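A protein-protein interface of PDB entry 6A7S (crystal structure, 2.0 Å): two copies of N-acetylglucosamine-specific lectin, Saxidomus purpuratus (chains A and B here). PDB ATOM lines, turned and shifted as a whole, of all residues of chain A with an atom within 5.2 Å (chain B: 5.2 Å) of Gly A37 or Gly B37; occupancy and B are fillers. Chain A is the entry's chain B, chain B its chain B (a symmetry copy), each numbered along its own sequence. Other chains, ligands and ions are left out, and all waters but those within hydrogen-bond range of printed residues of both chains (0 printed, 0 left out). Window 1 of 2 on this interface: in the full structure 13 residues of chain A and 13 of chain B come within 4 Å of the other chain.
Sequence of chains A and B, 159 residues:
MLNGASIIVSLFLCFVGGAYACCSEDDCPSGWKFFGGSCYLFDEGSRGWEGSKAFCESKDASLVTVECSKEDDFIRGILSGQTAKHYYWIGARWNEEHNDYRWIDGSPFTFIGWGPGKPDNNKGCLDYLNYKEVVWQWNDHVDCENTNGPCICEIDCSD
The backbone carbonyl oxygen (O) of Gly A37 sits at hydrogen-bond distance from the backbone NH (N) of Cys A22.
The backbone NH of Cys A22 sits at hydrogen-bond distance from the backbone carbonyl oxygen of Asp A156.
N of Cys A23 lies within hydrogen-bond range of O of Gly A37.
The backbone NH (N) of Cys B22 is in hydrogen-bond range of the backbone carbonyl oxygen (O) of Gly B37.
The backbone NH of Cys B22 sits at hydrogen-bond distance from the backbone carbonyl oxygen of Asp B156 (3.0 Å).
The backbone carbonyl oxygen (O) of Gly B37 is in hydrogen-bond range of the backbone NH (N) of Cys B23 (2.9 Å).
Cys A22 touches Phe B35.
Cys A22 touches Gly B36 (N to O, 3.6 Å).
Cys A23 touches Gly B36 (O to CA, 3.2 Å).
O of Cys B22 touches CZ of Phe A35, at 3.5 Å.
O of Gly A36 touches N of Cys B22, at 3.6 Å.
Gly A36 touches Cys B23 (CA to O, 3.2 Å).
C of Gly A36 touches CA of Gly B37, at 3.5 Å.
Gly B36 touches Gly A37.
Gly A37 touches Gly B37 (CA to N, 3.6 Å).
Cys A22 touches Gly B36, and with the chains exchanged Gly A36 touches Cys B22.
Cys A23 touches Gly B36, and with the chains exchanged Gly A36 touches Cys B23.
Gly A36 touches Gly B37, and with the chains exchanged Gly A37 touches Gly B36.
Gly B37 touches its own counterpart, Gly A37.
Positions printed for both chains: 22, 23, 34, 35, 36, 37, 38, 39, 155 and 156.
Of the 9 pairs that touch across the chains among the printed residues, 9 have their exchanged pair printed and touching as well.
Gly A37 touches two residues of chain B.
Of chain A, only Gly A36 and Gly A37 come within 4 Å of Gly B37.
Of the printed residues of chain A, Phe B35 touches Cys A22.
Of the printed residues of chain B, Cys A22 touches Phe B35 (3.5 Å) and Gly B36 (3.6 Å).
Of the printed residues of chain B, Gly A36 touches Cys B22, Cys B23 and Gly B37.
Ser A38 touches none of the printed residues of chain B.
Cys B39 touches none of the printed residues of chain A.
The nearest residue of chain B that does not touch Gly A37 is Cys B23 (4.5 Å).
The nearest printed residue of chain A that does not touch Cys B23 is Gly A37 (4.5 Å).
Of the 10 printed residues of chain A, 5 touch a printed residue of chain B.
Printed residues of chain A that touch a printed residue of chain B: Cys A22, Cys A23, Phe A35, Gly A36 and Gly A37.
Along chain A the printed residues that touch a printed residue of chain B span positions 22 to 37.
Of the 10 printed residues of chain B, 5 touch a printed residue of chain A.
Among the printed residues, no Asp or Glu carboxylate lies within 4 Å of a Lys or Arg side-chain nitrogen of the other chain.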
ATOM      1  N   CYS A  22      25.969 -10.636  -7.375  1.00  0.00           N
ATOM      2  CA  CYS A  22      25.585 -11.098  -8.688  1.00  0.00           C
ATOM      3  C   CYS A  22      26.272 -12.427  -8.949  1.00  0.00           C
ATOM      4  O   CYS A  22      26.110 -13.002 -10.022  1.00  0.00           O
ATOM      5  CB  CYS A  22      25.959 -10.043  -9.724  1.00  0.00           C
ATOM      6  SG  CYS A  22      25.158  -8.452  -9.380  1.00  0.00           S
ATOM      7  N   CYS A  23      27.027 -12.937  -7.956  1.00  0.00           N
ATOM      8  CA  CYS A  23      27.716 -14.209  -8.150  1.00  0.00           C
ATOM      9  C   CYS A  23      26.725 -15.350  -8.098  1.00  0.00           C
ATOM     10  O   CYS A  23      25.708 -15.283  -7.440  1.00  0.00           O
ATOM     11  CB  CYS A  23      28.793 -14.496  -7.100  1.00  0.00           C
ATOM     12  SG  CYS A  23      30.063 -13.224  -6.969  1.00  0.00           S
ATOM     13  N   PHE A  34      30.561 -19.728  -1.547  1.00  0.00           N
ATOM     14  CA  PHE A  34      29.387 -19.036  -2.113  1.00  0.00           C
ATOM     15  C   PHE A  34      28.357 -18.808  -1.012  1.00  0.00           C
ATOM     16  O   PHE A  34      27.980 -19.729  -0.303  1.00  0.00           O
ATOM     17  CB  PHE A  34      28.723 -19.805  -3.273  1.00  0.00           C
ATOM     18  CG  PHE A  34      27.510 -19.082  -3.827  1.00  0.00           C
ATOM     19  CD1 PHE A  34      27.661 -17.894  -4.553  1.00  0.00           C
ATOM     20  CD2 PHE A  34      26.215 -19.529  -3.569  1.00  0.00           C
ATOM     21  CE1 PHE A  34      26.554 -17.175  -4.999  1.00  0.00           C
ATOM     22  CE2 PHE A  34      25.108 -18.800  -4.011  1.00  0.00           C
ATOM     23  CZ  PHE A  34      25.275 -17.627  -4.727  1.00  0.00           C
ATOM     24  N   PHE A  35      27.902 -17.571  -0.888  1.00  0.00           N
ATOM     25  CA  PHE A  35      26.712 -17.279  -0.114  1.00  0.00           C
ATOM     26  C   PHE A  35      26.070 -16.007  -0.647  1.00  0.00           C
ATOM     27  O   PHE A  35      26.719 -14.971  -0.733  1.00  0.00           O
ATOM     28  CB  PHE A  35      27.001 -17.052   1.376  1.00  0.00           C
ATOM     29  CG  PHE A  35      25.796 -16.560   2.127  1.00  0.00           C
ATOM     30  CD1 PHE A  35      24.843 -17.457   2.571  1.00  0.00           C
ATOM     31  CD2 PHE A  35      25.538 -15.196   2.256  1.00  0.00           C
ATOM     32  CE1 PHE A  35      23.675 -17.017   3.179  1.00  0.00           C
ATOM     33  CE2 PHE A  35      24.364 -14.755   2.856  1.00  0.00           C
ATOM     34  CZ  PHE A  35      23.453 -15.666   3.348  1.00  0.00           C
ATOM     35  N   GLY A  36      24.763 -16.078  -0.928  1.00  0.00           N
ATOM     36  CA  GLY A  36      23.964 -14.852  -0.990  1.00  0.00           C
ATOM     37  C   GLY A  36      24.396 -13.896  -2.072  1.00  0.00           C
ATOM     38  O   GLY A  36      24.263 -12.676  -1.913  1.00  0.00           O
ATOM     39  N   GLY A  37      24.885 -14.453  -3.183  1.00  0.00           N
ATOM     40  CA  GLY A  37      25.284 -13.636  -4.302  1.00  0.00           C
ATOM     41  C   GLY A  37      26.716 -13.136  -4.216  1.00  0.00           C
ATOM     42  O   GLY A  37      27.134 -12.348  -5.089  1.00  0.00           O
ATOM     43  N   SER A  38      27.486 -13.611  -3.213  1.00  0.00           N
ATOM     44  CA  SER A  38      28.876 -13.221  -3.057  1.00  0.00           C
ATOM     45  C   SER A  38      29.754 -14.473  -2.984  1.00  0.00           C
ATOM     46  O   SER A  38      29.277 -15.578  -2.655  1.00  0.00           O
ATOM     47  CB  SER A  38      29.060 -12.340  -1.860  1.00  0.00           C
ATOM     48  OG  SER A  38      28.709 -11.014  -2.126  1.00  0.00           O
ATOM     49  N   CYS A  39      31.038 -14.309  -3.350  1.00  0.00           N
ATOM     50  CA  CYS A  39      32.050 -15.319  -3.102  1.00  0.00           C
ATOM     51  C   CYS A  39      32.989 -14.789  -1.997  1.00  0.00           C
ATOM     52  O   CYS A  39      33.314 -13.603  -1.955  1.00  0.00           O
ATOM     53  CB  CYS A  39      32.809 -15.665  -4.368  1.00  0.00           C
ATOM     54  SG  CYS A  39      31.738 -16.445  -5.607  1.00  0.00           S
ATOM     55  N   ILE A 155      33.936 -11.004  -3.020  1.00  0.00           N
ATOM     56  CA  ILE A 155      33.582 -10.477  -4.361  1.00  0.00           C
ATOM     57  C   ILE A 155      32.079 -10.668  -4.594  1.00  0.00           C
ATOM     58  O   ILE A 155      31.473 -11.666  -4.183  1.00  0.00           O
ATOM     59  CB  ILE A 155      34.395 -11.162  -5.480  1.00  0.00           C
ATOM     60  CG1 ILE A 155      34.120 -12.662  -5.595  1.00  0.00           C
ATOM     61  CG2 ILE A 155      35.872 -10.848  -5.281  1.00  0.00           C
ATOM     62  CD1 ILE A 155      34.752 -13.365  -6.819  1.00  0.00           C
ATOM     63  N   ASP A 156      31.504  -9.756  -5.360  1.00  0.00           N
ATOM     64  CA  ASP A 156      30.109  -9.909  -5.759  1.00  0.00           C
ATOM     65  C   ASP A 156      29.917  -9.994  -7.289  1.00  0.00           C
ATOM     66  O   ASP A 156      28.818  -9.838  -7.758  1.00  0.00           O
ATOM     67  CB  ASP A 156      29.338  -8.756  -5.167  1.00  0.00           C
ATOM     68  CG  ASP A 156      29.633  -7.443  -5.843  1.00  0.00           C
ATOM     69  OD1 ASP A 156      30.416  -7.435  -6.804  1.00  0.00           O
ATOM     70  OD2 ASP A 156      29.058  -6.455  -5.395  1.00  0.00           O
ATOM     71  N   CYS B  22      21.377 -11.250  -0.380  1.00  0.00           N
ATOM     72  CA  CYS B  22      21.654 -12.109   0.746  1.00  0.00           C
ATOM     73  C   CYS B  22      20.759 -13.333   0.648  1.00  0.00           C
ATOM     74  O   CYS B  22      20.805 -14.199   1.518  1.00  0.00           O
ATOM     75  CB  CYS B  22      21.428 -11.334   2.041  1.00  0.00           C
ATOM     76  SG  CYS B  22      22.479  -9.858   2.129  1.00  0.00           S
ATOM     77  N   CYS B  23      19.956 -13.425  -0.430  1.00  0.00           N
ATOM     78  CA  CYS B  23      19.070 -14.575  -0.577  1.00  0.00           C
ATOM     79  C   CYS B  23      19.870 -15.800  -0.963  1.00  0.00           C
ATOM     80  O   CYS B  23      20.899 -15.716  -1.600  1.00  0.00           O
ATOM     81  CB  CYS B  23      17.986 -14.389  -1.642  1.00  0.00           C
ATOM     82  SG  CYS B  23      16.936 -12.946  -1.390  1.00  0.00           S
ATOM     83  N   PHE B  34      15.536 -17.546  -8.379  1.00  0.00           N
ATOM     84  CA  PHE B  34      16.792 -17.230  -7.670  1.00  0.00           C
ATOM     85  C   PHE B  34      17.869 -16.875  -8.689  1.00  0.00           C
ATOM     86  O   PHE B  34      18.112 -17.612  -9.632  1.00  0.00           O
ATOM     87  CB  PHE B  34      17.300 -18.383  -6.781  1.00  0.00           C
ATOM     88  CG  PHE B  34      18.600 -18.042  -6.077  1.00  0.00           C
ATOM     89  CD1 PHE B  34      18.622 -17.090  -5.049  1.00  0.00           C
ATOM     90  CD2 PHE B  34      19.813 -18.600  -6.476  1.00  0.00           C
ATOM     91  CE1 PHE B  34      19.819 -16.706  -4.448  1.00  0.00           C
ATOM     92  CE2 PHE B  34      21.011 -18.204  -5.876  1.00  0.00           C
ATOM     93  CZ  PHE B  34      21.016 -17.262  -4.862  1.00  0.00           C
ATOM     94  N   PHE B  35      18.517 -15.739  -8.478  1.00  0.00           N
ATOM     95  CA  PHE B  35      19.755 -15.437  -9.168  1.00  0.00           C
ATOM     96  C   PHE B  35      20.578 -14.479  -8.320  1.00  0.00           C
ATOM     97  O   PHE B  35      20.100 -13.418  -7.939  1.00  0.00           O
ATOM     98  CB  PHE B  35      19.539 -14.767 -10.532  1.00  0.00           C
ATOM     99  CG  PHE B  35      20.823 -14.285 -11.145  1.00  0.00           C
ATOM    100  CD1 PHE B  35      21.632 -15.164 -11.840  1.00  0.00           C
ATOM    101  CD2 PHE B  35      21.296 -12.996 -10.901  1.00  0.00           C
ATOM    102  CE1 PHE B  35      22.868 -14.764 -12.329  1.00  0.00           C
ATOM    103  CE2 PHE B  35      22.539 -12.599 -11.382  1.00  0.00           C
ATOM    104  CZ  PHE B  35      23.304 -13.471 -12.126  1.00  0.00           C
ATOM    105  N   GLY B  36      21.851 -14.830  -8.100  1.00  0.00           N
ATOM    106  CA  GLY B  36      22.832 -13.811  -7.721  1.00  0.00           C
ATOM    107  C   GLY B  36      22.533 -13.133  -6.408  1.00  0.00           C
ATOM    108  O   GLY B  36      22.860 -11.954  -6.229  1.00  0.00           O
ATOM    109  N   GLY B  37      21.937 -13.889  -5.483  1.00  0.00           N
ATOM    110  CA  GLY B  37      21.647 -13.359  -4.173  1.00  0.00           C
ATOM    111  C   GLY B  37      20.315 -12.635  -4.087  1.00  0.00           C
ATOM    112  O   GLY B  37      20.007 -12.061  -3.021  1.00  0.00           O
ATOM    113  N   SER B  38      19.502 -12.688  -5.165  1.00  0.00           N
ATOM    114  CA  SER B  38      18.195 -12.055  -5.176  1.00  0.00           C
ATOM    115  C   SER B  38      17.132 -13.083  -5.571  1.00  0.00           C
ATOM    116  O   SER B  38      17.435 -14.117  -6.202  1.00  0.00           O
ATOM    117  CB  SER B  38      18.179 -10.861  -6.081  1.00  0.00           C
ATOM    118  OG  SER B  38      18.730  -9.733  -5.469  1.00  0.00           O
ATOM    119  N   CYS B  39      15.882 -12.826  -5.145  1.00  0.00           N
ATOM    120  CA  CYS B  39      14.729 -13.555  -5.639  1.00  0.00           C
ATOM    121  C   CYS B  39      13.910 -12.601  -6.534  1.00  0.00           C
ATOM    122  O   CYS B  39      13.778 -11.413  -6.241  1.00  0.00           O
ATOM    123  CB  CYS B  39      13.897 -14.112  -4.500  1.00  0.00           C
ATOM    124  SG  CYS B  39      14.803 -15.361  -3.547  1.00  0.00           S
ATOM    125  N   ILE B 155      13.551  -9.143  -4.489  1.00  0.00           N
ATOM    126  CA  ILE B 155      13.954  -9.068  -3.063  1.00  0.00           C
ATOM    127  C   ILE B 155      15.403  -9.550  -2.926  1.00  0.00           C
ATOM    128  O   ILE B 155      15.852 -10.479  -3.609  1.00  0.00           O
ATOM    129  CB  ILE B 155      13.019  -9.896  -2.158  1.00  0.00           C
ATOM    130  CG1 ILE B 155      13.050 -11.394  -2.466  1.00  0.00           C
ATOM    131  CG2 ILE B 155      11.615  -9.309  -2.230  1.00  0.00           C
ATOM    132  CD1 ILE B 155      12.288 -12.296  -1.468  1.00  0.00           C
ATOM    133  N   ASP B 156      16.097  -8.986  -1.952  1.00  0.00           N
ATOM    134  CA  ASP B 156      17.441  -9.462  -1.642  1.00  0.00           C
ATOM    135  C   ASP B 156      17.584  -9.993  -0.198  1.00  0.00           C
ATOM    136  O   ASP B 156      18.683 -10.148   0.271  1.00  0.00           O
ATOM    137  CB  ASP B 156      18.398  -8.328  -1.910  1.00  0.00           C
ATOM    138  CG  ASP B 156      18.299  -7.221  -0.894  1.00  0.00           C
ATOM    139  OD1 ASP B 156      17.506  -7.354   0.050  1.00  0.00           O
ATOM    140  OD2 ASP B 156      19.033  -6.252  -1.065  1.00  0.00           O
